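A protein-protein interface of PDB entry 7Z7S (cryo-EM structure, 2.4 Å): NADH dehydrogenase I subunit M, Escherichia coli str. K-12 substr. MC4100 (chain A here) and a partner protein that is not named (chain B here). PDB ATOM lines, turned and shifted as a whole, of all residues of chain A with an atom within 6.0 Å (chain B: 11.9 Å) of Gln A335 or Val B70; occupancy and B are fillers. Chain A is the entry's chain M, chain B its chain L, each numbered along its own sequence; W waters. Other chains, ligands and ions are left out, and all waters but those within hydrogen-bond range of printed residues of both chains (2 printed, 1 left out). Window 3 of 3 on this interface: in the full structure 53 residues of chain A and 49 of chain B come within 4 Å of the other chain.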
ATOM      1  N   GLY A 333     -21.826  10.003 -12.685  1.00  0.00           N
ATOM      2  CA  GLY A 333     -22.333  10.833 -11.613  1.00  0.00           C
ATOM      3  C   GLY A 333     -22.679  12.250 -11.996  1.00  0.00           C
ATOM      4  O   GLY A 333     -22.741  13.114 -11.122  1.00  0.00           O
ATOM      5  N   SER A 334     -22.919  12.517 -13.274  1.00  0.00           N
ATOM      6  CA  SER A 334     -23.204  13.857 -13.761  1.00  0.00           C
ATOM      7  C   SER A 334     -24.632  13.932 -14.278  1.00  0.00           C
ATOM      8  O   SER A 334     -25.095  13.029 -14.975  1.00  0.00           O
ATOM      9  CB  SER A 334     -22.227  14.258 -14.865  1.00  0.00           C
ATOM     10  OG  SER A 334     -22.736  15.321 -15.644  1.00  0.00           O
ATOM     11  N   GLN A 335     -25.324  15.011 -13.916  1.00  0.00           N
ATOM     12  CA  GLN A 335     -26.706  15.198 -14.346  1.00  0.00           C
ATOM     13  C   GLN A 335     -26.801  15.384 -15.856  1.00  0.00           C
ATOM     14  O   GLN A 335     -27.697  14.830 -16.506  1.00  0.00           O
ATOM     15  CB  GLN A 335     -27.303  16.399 -13.620  1.00  0.00           C
ATOM     16  CG  GLN A 335     -28.654  16.817 -14.128  1.00  0.00           C
ATOM     17  CD  GLN A 335     -29.750  16.214 -13.308  1.00  0.00           C
ATOM     18  OE1 GLN A 335     -29.492  15.659 -12.246  1.00  0.00           O
ATOM     19  NE2 GLN A 335     -30.982  16.304 -13.793  1.00  0.00           N
ATOM     20  N   LEU A 336     -25.878  16.161 -16.424  1.00  0.00           N
ATOM     21  CA  LEU A 336     -25.870  16.422 -17.858  1.00  0.00           C
ATOM     22  C   LEU A 336     -25.654  15.145 -18.658  1.00  0.00           C
ATOM     23  O   LEU A 336     -26.350  14.896 -19.650  1.00  0.00           O
ATOM     24  CB  LEU A 336     -24.785  17.450 -18.171  1.00  0.00           C
ATOM     25  CG  LEU A 336     -24.595  17.936 -19.599  1.00  0.00           C
ATOM     26  CD1 LEU A 336     -25.896  18.446 -20.148  1.00  0.00           C
ATOM     27  CD2 LEU A 336     -23.544  19.016 -19.610  1.00  0.00           C
ATOM     28  N   ALA A 337     -24.717  14.306 -18.222  1.00  0.00           N
ATOM     29  CA  ALA A 337     -24.467  13.056 -18.921  1.00  0.00           C
ATOM     30  C   ALA A 337     -25.610  12.068 -18.742  1.00  0.00           C
ATOM     31  O   ALA A 337     -25.900  11.299 -19.660  1.00  0.00           O
ATOM     32  CB  ALA A 337     -23.153  12.445 -18.451  1.00  0.00           C
ATOM     33  N   TYR A 338     -26.278  12.080 -17.586  1.00  0.00           N
ATOM     34  CA  TYR A 338     -27.431  11.204 -17.388  1.00  0.00           C
ATOM     35  C   TYR A 338     -28.591  11.604 -18.292  1.00  0.00           C
ATOM     36  O   TYR A 338     -29.271  10.741 -18.865  1.00  0.00           O
ATOM     37  CB  TYR A 338     -27.890  11.243 -15.934  1.00  0.00           C
ATOM     38  CG  TYR A 338     -27.029  10.532 -14.919  1.00  0.00           C
ATOM     39  CD1 TYR A 338     -25.829   9.945 -15.274  1.00  0.00           C
ATOM     40  CD2 TYR A 338     -27.428  10.456 -13.594  1.00  0.00           C
ATOM     41  CE1 TYR A 338     -25.056   9.317 -14.346  1.00  0.00           C
ATOM     42  CE2 TYR A 338     -26.658   9.819 -12.660  1.00  0.00           C
ATOM     43  CZ  TYR A 338     -25.473   9.249 -13.041  1.00  0.00           C
ATOM     44  OH  TYR A 338     -24.694   8.608 -12.112  1.00  0.00           O
ATOM     45  N   GLN A 339     -28.839  12.909 -18.417  1.00  0.00           N
ATOM     46  CA  GLN A 339     -29.879  13.384 -19.325  1.00  0.00           C
ATOM     47  C   GLN A 339     -29.534  13.060 -20.771  1.00  0.00           C
ATOM     48  O   GLN A 339     -30.413  12.682 -21.561  1.00  0.00           O
ATOM     49  CB  GLN A 339     -30.086  14.884 -19.139  1.00  0.00           C
ATOM     50  CG  GLN A 339     -30.721  15.257 -17.823  1.00  0.00           C
ATOM     51  CD  GLN A 339     -32.221  15.155 -17.870  1.00  0.00           C
ATOM     52  OE1 GLN A 339     -32.781  14.067 -17.792  1.00  0.00           O
ATOM     53  NE2 GLN A 339     -32.885  16.291 -18.001  1.00  0.00           N
ATOM     54  N   GLY A 340     -28.255  13.189 -21.130  1.00  0.00           N
ATOM     55  CA  GLY A 340     -27.820  12.751 -22.442  1.00  0.00           C
ATOM     56  C   GLY A 340     -28.017  11.264 -22.656  1.00  0.00           C
ATOM     57  O   GLY A 340     -28.340  10.831 -23.758  1.00  0.00           O
ATOM     58  N   MET A 409     -24.457  15.551 -25.183  1.00  0.00           N
ATOM     59  CA  MET A 409     -24.666  15.875 -23.776  1.00  0.00           C
ATOM     60  C   MET A 409     -23.955  14.872 -22.876  1.00  0.00           C
ATOM     61  O   MET A 409     -23.392  15.251 -21.834  1.00  0.00           O
ATOM     62  CB  MET A 409     -26.160  15.945 -23.480  1.00  0.00           C
ATOM     63  CG  MET A 409     -26.700  17.357 -23.616  1.00  0.00           C
ATOM     64  SD  MET A 409     -28.487  17.514 -23.521  1.00  0.00           S
ATOM     65  CE  MET A 409     -28.841  16.318 -22.263  1.00  0.00           C
ATOM     66  N   GLN A 483     -36.373  19.578 -25.390  1.00  0.00           N
ATOM     67  CA  GLN A 483     -36.720  20.083 -24.064  1.00  0.00           C
ATOM     68  C   GLN A 483     -37.890  19.379 -23.376  1.00  0.00           C
ATOM     69  O   GLN A 483     -37.806  19.208 -22.150  1.00  0.00           O
ATOM     70  CB  GLN A 483     -36.968  21.594 -24.129  1.00  0.00           C
ATOM     71  CG  GLN A 483     -36.718  22.300 -22.812  1.00  0.00           C
ATOM     72  CD  GLN A 483     -35.385  21.932 -22.199  1.00  0.00           C
ATOM     73  OE1 GLN A 483     -34.344  22.056 -22.833  1.00  0.00           O
ATOM     74  NE2 GLN A 483     -35.413  21.479 -20.957  1.00  0.00           N
ATOM     75  N   LEU A 486     -36.353  16.293 -21.935  1.00  0.00           N
ATOM     76  CA  LEU A 486     -35.428  16.615 -20.856  1.00  0.00           C
ATOM     77  C   LEU A 486     -36.168  17.038 -19.595  1.00  0.00           C
ATOM     78  O   LEU A 486     -35.721  16.750 -18.481  1.00  0.00           O
ATOM     79  CB  LEU A 486     -34.470  17.713 -21.304  1.00  0.00           C
ATOM     80  CG  LEU A 486     -33.426  17.285 -22.328  1.00  0.00           C
ATOM     81  CD1 LEU A 486     -32.661  18.487 -22.833  1.00  0.00           C
ATOM     82  CD2 LEU A 486     -32.496  16.281 -21.702  1.00  0.00           C
ATOM     83  N   SER A 489     -37.820  13.825 -17.683  1.00  0.00           N
ATOM     84  CA  SER A 489     -36.934  12.956 -16.925  1.00  0.00           C
ATOM     85  C   SER A 489     -36.024  13.709 -15.967  1.00  0.00           C
ATOM     86  O   SER A 489     -35.166  13.087 -15.343  1.00  0.00           O
ATOM     87  CB  SER A 489     -36.082  12.118 -17.873  1.00  0.00           C
ATOM     88  OG  SER A 489     -35.174  12.932 -18.590  1.00  0.00           O
ATOM     89  N   HIS A 490     -36.194  15.025 -15.834  1.00  0.00           N
ATOM     90  CA  HIS A 490     -35.256  15.831 -15.057  1.00  0.00           C
ATOM     91  C   HIS A 490     -35.292  15.488 -13.572  1.00  0.00           C
ATOM     92  O   HIS A 490     -34.241  15.408 -12.927  1.00  0.00           O
ATOM     93  CB  HIS A 490     -35.554  17.314 -15.268  1.00  0.00           C
ATOM     94  CG  HIS A 490     -35.126  18.182 -14.130  1.00  0.00           C
ATOM     95  ND1 HIS A 490     -36.006  18.645 -13.177  1.00  0.00           N
ATOM     96  CD2 HIS A 490     -33.910  18.665 -13.786  1.00  0.00           C
ATOM     97  CE1 HIS A 490     -35.351  19.377 -12.295  1.00  0.00           C
ATOM     98  NE2 HIS A 490     -34.078  19.406 -12.642  1.00  0.00           N
ATOM     99  N   SER A 491     -36.484  15.279 -13.013  1.00  0.00           N
ATOM    100  CA  SER A 491     -36.599  15.025 -11.580  1.00  0.00           C
ATOM    101  C   SER A 491     -36.055  13.651 -11.204  1.00  0.00           C
ATOM    102  O   SER A 491     -35.356  13.513 -10.194  1.00  0.00           O
ATOM    103  CB  SER A 491     -38.056  15.164 -11.148  1.00  0.00           C
ATOM    104  OG  SER A 491     -38.219  14.806  -9.792  1.00  0.00           O
ATOM    105  N   ILE A 493     -33.814  11.771 -12.877  1.00  0.00           N
ATOM    106  CA  ILE A 493     -32.370  11.821 -13.058  1.00  0.00           C
ATOM    107  C   ILE A 493     -31.714  12.593 -11.926  1.00  0.00           C
ATOM    108  O   ILE A 493     -30.654  12.203 -11.426  1.00  0.00           O
ATOM    109  CB  ILE A 493     -32.051  12.422 -14.441  1.00  0.00           C
ATOM    110  CG1 ILE A 493     -32.393  11.421 -15.550  1.00  0.00           C
ATOM    111  CG2 ILE A 493     -30.644  12.954 -14.520  1.00  0.00           C
ATOM    112  CD1 ILE A 493     -31.799  10.049 -15.347  1.00  0.00           C
ATOM    113  N   GLY A 494     -32.345  13.685 -11.491  1.00  0.00           N
ATOM    114  CA  GLY A 494     -31.816  14.440 -10.370  1.00  0.00           C
ATOM    115  C   GLY A 494     -31.791  13.643  -9.084  1.00  0.00           C
ATOM    116  O   GLY A 494     -30.815  13.697  -8.333  1.00  0.00           O
ATOM    117  N   ASN A 495     -32.855  12.881  -8.822  1.00  0.00           N
ATOM    118  CA  ASN A 495     -32.902  12.034  -7.632  1.00  0.00           C
ATOM    119  C   ASN A 495     -31.815  10.971  -7.670  1.00  0.00           C
ATOM    120  O   ASN A 495     -31.109  10.755  -6.678  1.00  0.00           O
ATOM    121  CB  ASN A 495     -34.274  11.376  -7.514  1.00  0.00           C
ATOM    122  CG  ASN A 495     -35.340  12.337  -7.069  1.00  0.00           C
ATOM    123  OD1 ASN A 495     -35.058  13.324  -6.403  1.00  0.00           O
ATOM    124  ND2 ASN A 495     -36.577  12.054  -7.434  1.00  0.00           N
ATOM    125  N   GLN A 497     -28.973  10.959  -9.440  1.00  0.00           N
ATOM    126  CA  GLN A 497     -27.655  11.578  -9.354  1.00  0.00           C
ATOM    127  C   GLN A 497     -27.346  12.060  -7.942  1.00  0.00           C
ATOM    128  O   GLN A 497     -26.221  11.891  -7.460  1.00  0.00           O
ATOM    129  CB  GLN A 497     -27.559  12.736 -10.345  1.00  0.00           C
ATOM    130  CG  GLN A 497     -26.149  13.236 -10.573  1.00  0.00           C
ATOM    131  CD  GLN A 497     -25.823  14.456  -9.743  1.00  0.00           C
ATOM    132  OE1 GLN A 497     -26.714  15.181  -9.308  1.00  0.00           O
ATOM    133  NE2 GLN A 497     -24.540  14.687  -9.512  1.00  0.00           N
ATOM    134  N   GLN A 498     -28.327  12.663  -7.263  1.00  0.00           N
ATOM    135  CA  GLN A 498     -28.094  13.146  -5.908  1.00  0.00           C
ATOM    136  C   GLN A 498     -27.893  11.996  -4.934  1.00  0.00           C
ATOM    137  O   GLN A 498     -27.056  12.086  -4.032  1.00  0.00           O
ATOM    138  CB  GLN A 498     -29.248  14.038  -5.460  1.00  0.00           C
ATOM    139  CG  GLN A 498     -29.118  15.473  -5.931  1.00  0.00           C
ATOM    140  CD  GLN A 498     -27.743  16.049  -5.654  1.00  0.00           C
ATOM    141  OE1 GLN A 498     -27.271  16.046  -4.519  1.00  0.00           O
ATOM    142  NE2 GLN A 498     -27.091  16.546  -6.697  1.00  0.00           N
ATOM    143  N   THR B  66     -35.043  27.748 -26.848  1.00  0.00           N
ATOM    144  CA  THR B  66     -33.920  27.203 -26.098  1.00  0.00           C
ATOM    145  C   THR B  66     -33.700  25.763 -26.535  1.00  0.00           C
ATOM    146  O   THR B  66     -34.607  24.932 -26.426  1.00  0.00           O
ATOM    147  CB  THR B  66     -34.165  27.275 -24.593  1.00  0.00           C
ATOM    148  OG1 THR B  66     -34.474  28.621 -24.224  1.00  0.00           O
ATOM    149  CG2 THR B  66     -32.928  26.828 -23.841  1.00  0.00           C
ATOM    150  N   TRP B  67     -32.498  25.476 -27.031  1.00  0.00           N
ATOM    151  CA  TRP B  67     -32.210  24.155 -27.574  1.00  0.00           C
ATOM    152  C   TRP B  67     -32.094  23.122 -26.464  1.00  0.00           C
ATOM    153  O   TRP B  67     -32.826  22.126 -26.448  1.00  0.00           O
ATOM    154  CB  TRP B  67     -30.930  24.212 -28.405  1.00  0.00           C
ATOM    155  CG  TRP B  67     -30.758  23.078 -29.341  1.00  0.00           C
ATOM    156  CD1 TRP B  67     -31.668  22.111 -29.636  1.00  0.00           C
ATOM    157  CD2 TRP B  67     -29.596  22.787 -30.114  1.00  0.00           C
ATOM    158  NE1 TRP B  67     -31.143  21.232 -30.546  1.00  0.00           N
ATOM    159  CE2 TRP B  67     -29.872  21.628 -30.860  1.00  0.00           C
ATOM    160  CE3 TRP B  67     -28.348  23.399 -30.255  1.00  0.00           C
ATOM    161  CZ2 TRP B  67     -28.944  21.062 -31.724  1.00  0.00           C
ATOM    162  CZ3 TRP B  67     -27.433  22.841 -31.113  1.00  0.00           C
ATOM    163  CH2 TRP B  67     -27.733  21.684 -31.839  1.00  0.00           C
ATOM    164  N   MET B  68     -31.184  23.338 -25.522  1.00  0.00           N
ATOM    165  CA  MET B  68     -30.998  22.421 -24.410  1.00  0.00           C
ATOM    166  C   MET B  68     -30.923  23.202 -23.109  1.00  0.00           C
ATOM    167  O   MET B  68     -30.417  24.323 -23.072  1.00  0.00           O
ATOM    168  CB  MET B  68     -29.728  21.583 -24.564  1.00  0.00           C
ATOM    169  CG  MET B  68     -29.733  20.619 -25.725  1.00  0.00           C
ATOM    170  SD  MET B  68     -28.086  20.450 -26.422  1.00  0.00           S
ATOM    171  CE  MET B  68     -28.470  19.997 -28.101  1.00  0.00           C
ATOM    172  N   SER B  69     -31.417  22.588 -22.037  1.00  0.00           N
ATOM    173  CA  SER B  69     -31.347  23.200 -20.712  1.00  0.00           C
ATOM    174  C   SER B  69     -31.289  22.076 -19.685  1.00  0.00           C
ATOM    175  O   SER B  69     -32.316  21.478 -19.359  1.00  0.00           O
ATOM    176  CB  SER B  69     -32.531  24.123 -20.466  1.00  0.00           C
ATOM    177  OG  SER B  69     -32.456  24.708 -19.182  1.00  0.00           O
ATOM    178  N   VAL B  70     -30.085  21.785 -19.200  1.00  0.00           N
ATOM    179  CA  VAL B  70     -29.858  20.832 -18.117  1.00  0.00           C
ATOM    180  C   VAL B  70     -28.999  21.552 -17.086  1.00  0.00           C
ATOM    181  O   VAL B  70     -27.775  21.630 -17.238  1.00  0.00           O
ATOM    182  CB  VAL B  70     -29.181  19.539 -18.592  1.00  0.00           C
ATOM    183  CG1 VAL B  70     -28.966  18.593 -17.425  1.00  0.00           C
ATOM    184  CG2 VAL B  70     -29.995  18.862 -19.669  1.00  0.00           C
ATOM    185  N   GLY B  71     -29.629  22.073 -16.040  1.00  0.00           N
ATOM    186  CA  GLY B  71     -28.886  22.730 -14.974  1.00  0.00           C
ATOM    187  C   GLY B  71     -28.233  24.010 -15.453  1.00  0.00           C
ATOM    188  O   GLY B  71     -28.899  24.941 -15.920  1.00  0.00           O
ATOM    189  N   ASP B  72     -26.909  24.070 -15.337  1.00  0.00           N
ATOM    190  CA  ASP B  72     -26.155  25.200 -15.861  1.00  0.00           C
ATOM    191  C   ASP B  72     -25.877  25.088 -17.353  1.00  0.00           C
ATOM    192  O   ASP B  72     -25.432  26.068 -17.958  1.00  0.00           O
ATOM    193  CB  ASP B  72     -24.835  25.344 -15.103  1.00  0.00           C
ATOM    194  CG  ASP B  72     -25.024  25.920 -13.715  1.00  0.00           C
ATOM    195  OD1 ASP B  72     -25.938  26.750 -13.533  1.00  0.00           O
ATOM    196  OD2 ASP B  72     -24.259  25.542 -12.806  1.00  0.00           O
ATOM    197  N   PHE B  73     -26.125  23.927 -17.956  1.00  0.00           N
ATOM    198  CA  PHE B  73     -25.925  23.716 -19.386  1.00  0.00           C
ATOM    199  C   PHE B  73     -27.127  24.288 -20.112  1.00  0.00           C
ATOM    200  O   PHE B  73     -28.162  23.642 -20.246  1.00  0.00           O
ATOM    201  CB  PHE B  73     -25.748  22.235 -19.689  1.00  0.00           C
ATOM    202  CG  PHE B  73     -25.409  21.935 -21.118  1.00  0.00           C
ATOM    203  CD1 PHE B  73     -24.114  22.064 -21.576  1.00  0.00           C
ATOM    204  CD2 PHE B  73     -26.387  21.507 -21.999  1.00  0.00           C
ATOM    205  CE1 PHE B  73     -23.798  21.781 -22.880  1.00  0.00           C
ATOM    206  CE2 PHE B  73     -26.076  21.222 -23.306  1.00  0.00           C
ATOM    207  CZ  PHE B  73     -24.778  21.358 -23.747  1.00  0.00           C
ATOM    208  N   ASN B  74     -26.998  25.521 -20.579  1.00  0.00           N
ATOM    209  CA  ASN B  74     -28.070  26.192 -21.303  1.00  0.00           C
ATOM    210  C   ASN B  74     -27.548  26.568 -22.680  1.00  0.00           C
ATOM    211  O   ASN B  74     -26.652  27.408 -22.800  1.00  0.00           O
ATOM    212  CB  ASN B  74     -28.568  27.416 -20.541  1.00  0.00           C
ATOM    213  CG  ASN B  74     -29.928  27.868 -21.006  1.00  0.00           C
ATOM    214  OD1 ASN B  74     -30.083  28.345 -22.126  1.00  0.00           O
ATOM    215  ND2 ASN B  74     -30.927  27.707 -20.152  1.00  0.00           N
ATOM    216  N   ILE B  75     -28.103  25.942 -23.711  1.00  0.00           N
ATOM    217  CA  ILE B  75     -27.730  26.198 -25.094  1.00  0.00           C
ATOM    218  C   ILE B  75     -28.968  26.704 -25.808  1.00  0.00           C
ATOM    219  O   ILE B  75     -29.997  26.017 -25.837  1.00  0.00           O
ATOM    220  CB  ILE B  75     -27.179  24.940 -25.780  1.00  0.00           C
ATOM    221  CG1 ILE B  75     -25.879  24.494 -25.108  1.00  0.00           C
ATOM    222  CG2 ILE B  75     -26.982  25.185 -27.263  1.00  0.00           C
ATOM    223  CD1 ILE B  75     -24.788  25.520 -25.144  1.00  0.00           C
ATOM    224  N   GLY B  76     -28.871  27.893 -26.388  1.00  0.00           N
ATOM    225  CA  GLY B  76     -29.995  28.529 -27.039  1.00  0.00           C
ATOM    226  C   GLY B  76     -29.938  28.411 -28.549  1.00  0.00           C
ATOM    227  O   GLY B  76     -28.869  28.393 -29.147  1.00  0.00           O
ATOM    228  N   LEU B 137     -22.439  25.657 -29.980  1.00  0.00           N
ATOM    229  CA  LEU B 137     -23.147  24.417 -30.291  1.00  0.00           C
ATOM    230  C   LEU B 137     -24.062  24.560 -31.505  1.00  0.00           C
ATOM    231  O   LEU B 137     -24.158  23.639 -32.323  1.00  0.00           O
ATOM    232  CB  LEU B 137     -23.940  23.943 -29.074  1.00  0.00           C
ATOM    233  CG  LEU B 137     -24.357  22.469 -29.087  1.00  0.00           C
ATOM    234  CD1 LEU B 137     -23.197  21.565 -29.453  1.00  0.00           C
ATOM    235  CD2 LEU B 137     -24.938  22.058 -27.757  1.00  0.00           C
ATOM    236  N   TYR B 189     -16.954  24.835 -22.251  1.00  0.00           N
ATOM    237  CA  TYR B 189     -18.080  24.744 -21.330  1.00  0.00           C
ATOM    238  C   TYR B 189     -17.624  24.331 -19.935  1.00  0.00           C
ATOM    239  O   TYR B 189     -18.171  24.807 -18.935  1.00  0.00           O
ATOM    240  CB  TYR B 189     -19.138  23.773 -21.843  1.00  0.00           C
ATOM    241  CG  TYR B 189     -20.210  23.538 -20.812  1.00  0.00           C
ATOM    242  CD1 TYR B 189     -21.077  24.558 -20.450  1.00  0.00           C
ATOM    243  CD2 TYR B 189     -20.321  22.320 -20.159  1.00  0.00           C
ATOM    244  CE1 TYR B 189     -22.040  24.363 -19.490  1.00  0.00           C
ATOM    245  CE2 TYR B 189     -21.278  22.119 -19.196  1.00  0.00           C
ATOM    246  CZ  TYR B 189     -22.133  23.144 -18.867  1.00  0.00           C
ATOM    247  OH  TYR B 189     -23.089  22.938 -17.908  1.00  0.00           O
ATOM    248  N   ASN B 190     -16.633  23.440 -19.841  1.00  0.00           N
ATOM    249  CA  ASN B 190     -16.152  23.018 -18.531  1.00  0.00           C
ATOM    250  C   ASN B 190     -15.458  24.152 -17.790  1.00  0.00           C
ATOM    251  O   ASN B 190     -15.519  24.211 -16.557  1.00  0.00           O
ATOM    252  CB  ASN B 190     -15.208  21.828 -18.677  1.00  0.00           C
ATOM    253  CG  ASN B 190     -14.797  21.248 -17.346  1.00  0.00           C
ATOM    254  OD1 ASN B 190     -15.606  21.131 -16.431  1.00  0.00           O
ATOM    255  ND2 ASN B 190     -13.529  20.884 -17.228  1.00  0.00           N
ATOM    256  N   GLY B 193     -18.604  27.630 -18.427  1.00  0.00           N
ATOM    257  CA  GLY B 193     -20.014  27.414 -18.196  1.00  0.00           C
ATOM    258  C   GLY B 193     -20.931  27.947 -19.270  1.00  0.00           C
ATOM    259  O   GLY B 193     -22.148  27.974 -19.064  1.00  0.00           O
ATOM    260  N   THR B 194     -20.389  28.375 -20.405  1.00  0.00           N
ATOM    261  CA  THR B 194     -21.196  28.936 -21.473  1.00  0.00           C
ATOM    262  C   THR B 194     -20.506  28.667 -22.799  1.00  0.00           C
ATOM    263  O   THR B 194     -19.299  28.429 -22.856  1.00  0.00           O
ATOM    264  CB  THR B 194     -21.422  30.441 -21.280  1.00  0.00           C
ATOM    265  OG1 THR B 194     -22.145  30.969 -22.395  1.00  0.00           O
ATOM    266  CG2 THR B 194     -20.097  31.167 -21.163  1.00  0.00           C
ATOM    267  N   LEU B 195     -21.293  28.699 -23.869  1.00  0.00           N
ATOM    268  CA  LEU B 195     -20.764  28.602 -25.217  1.00  0.00           C
ATOM    269  C   LEU B 195     -21.127  29.806 -26.071  1.00  0.00           C
ATOM    270  O   LEU B 195     -20.741  29.852 -27.241  1.00  0.00           O
ATOM    271  CB  LEU B 195     -21.249  27.312 -25.891  1.00  0.00           C
ATOM    272  CG  LEU B 195     -20.675  26.012 -25.319  1.00  0.00           C
ATOM    273  CD1 LEU B 195     -21.135  24.821 -26.123  1.00  0.00           C
ATOM    274  CD2 LEU B 195     -19.160  26.062 -25.263  1.00  0.00           C
HETATM  275  O   HOH W   1     -35.313  22.406 -26.850  1.00  0.00           O
HETATM  276  O   HOH W   2     -32.698  18.716 -17.314  1.00  0.00           O
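Water W2 bridges NE2 of Gln A339 and O of Ser B69. Water W1 lies within hydrogen-bond range of O of Trp B67, O of Thr B66 and N of Gln A483.
The backbone carbonyl oxygen (O) of Ile B75 is in hydrogen-bond range of the backbone NH (N) of Trp B67. N of Phe B73 is in hydrogen-bond range of OH of Tyr B189 (3.2 Å). The side-chain amide oxygen (OE1) of Gln A339 lies within hydrogen-bond range of the side-chain hydroxyl (OG) of Ser A489 (2.8 Å). The side-chain amide nitrogen of Gln A339 sits at hydrogen-bond distance from the backbone carbonyl oxygen of Leu A486, at 2.9 Å. The backbone carbonyl oxygen (O) of Met B68 sits at hydrogen-bond distance from the backbone NH (N) of Ile B75. The backbone NH (N) of Leu A336 sits close to the side-chain hydroxyl (OG) of Ser A334 (3.3 Å).
No residue of chain B comes within 4 Å of Gly A333. No residue of chain B comes within 4 Å of Ser A334. Gln A335 touches one residue of chain B. No residue of chain B comes within 4 Å of Ala A337. No residue of chain B comes within 4 Å of Tyr A338. Printed residues of chain B within 4 Å of Gln A339: Val B70 (3.8 Å). Of the printed residues of chain B, Met A409 touches Val B70 and Phe B73. No residue of chain B comes within 4 Å of Leu A486. No residue of chain B comes within 4 Å of His A490. No residue of chain B comes within 4 Å of Ile A493. No residue of chain B comes within 4 Å of Gln A497. Of the printed residues of chain A, Trp B67 touches Gln A483. Printed residues of chain A within 4 Å of Ser B69: Gln A483. Val B70 touches just these residues of chain A: Gln A335, Leu A336, Gln A339 and Met A409. Asp B72 touches none of the printed residues of chain A. Gly B76 touches none of the printed residues of chain A. Of the printed residues of chain A, Tyr B189 touches Leu A336 (3.9 Å). The nearest printed residue of chain B that does not touch Met A409 is Met B68 (4.01 Å).
The side-chain amide oxygen of Gln A483 is in hydrogen-bond range of the backbone NH of Ser B69, 3.1 Å away.
Val B70 touches Gln A335 (CG1 to CG, 3.8 Å). Leu A336 touches Val B70. Leu A336 touches Phe B73 (CD1 to CD2, 3.6 Å). CD2 of Leu A336 touches CE2 of Tyr B189 (3.9 Å). Gln A339 touches Val B70. Val B70 touches Met A409 (CG2 to CE, 3.8 Å). Met A409 touches Phe B73. OE1 of Gln A483 touches O of Trp B67, at 3.9 Å. OE1 of Gln A483 touches C of Met B68 (3.6 Å).
Printed residues of chain B that touch a printed residue of chain A: Trp B67, Met B68, Ser B69, Val B70, Phe B73 and Tyr B189. Hydrophobic or aromatic side chains of chain A within 4 Å of the printed part of chain B: Leu A336 and Met A409. Among the printed residues, 10 pairs touch across the chains. Among the printed residues, no Asp or Glu carboxylate lies within 4 Å of a Lys or Arg side-chain nitrogen of the other chain.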
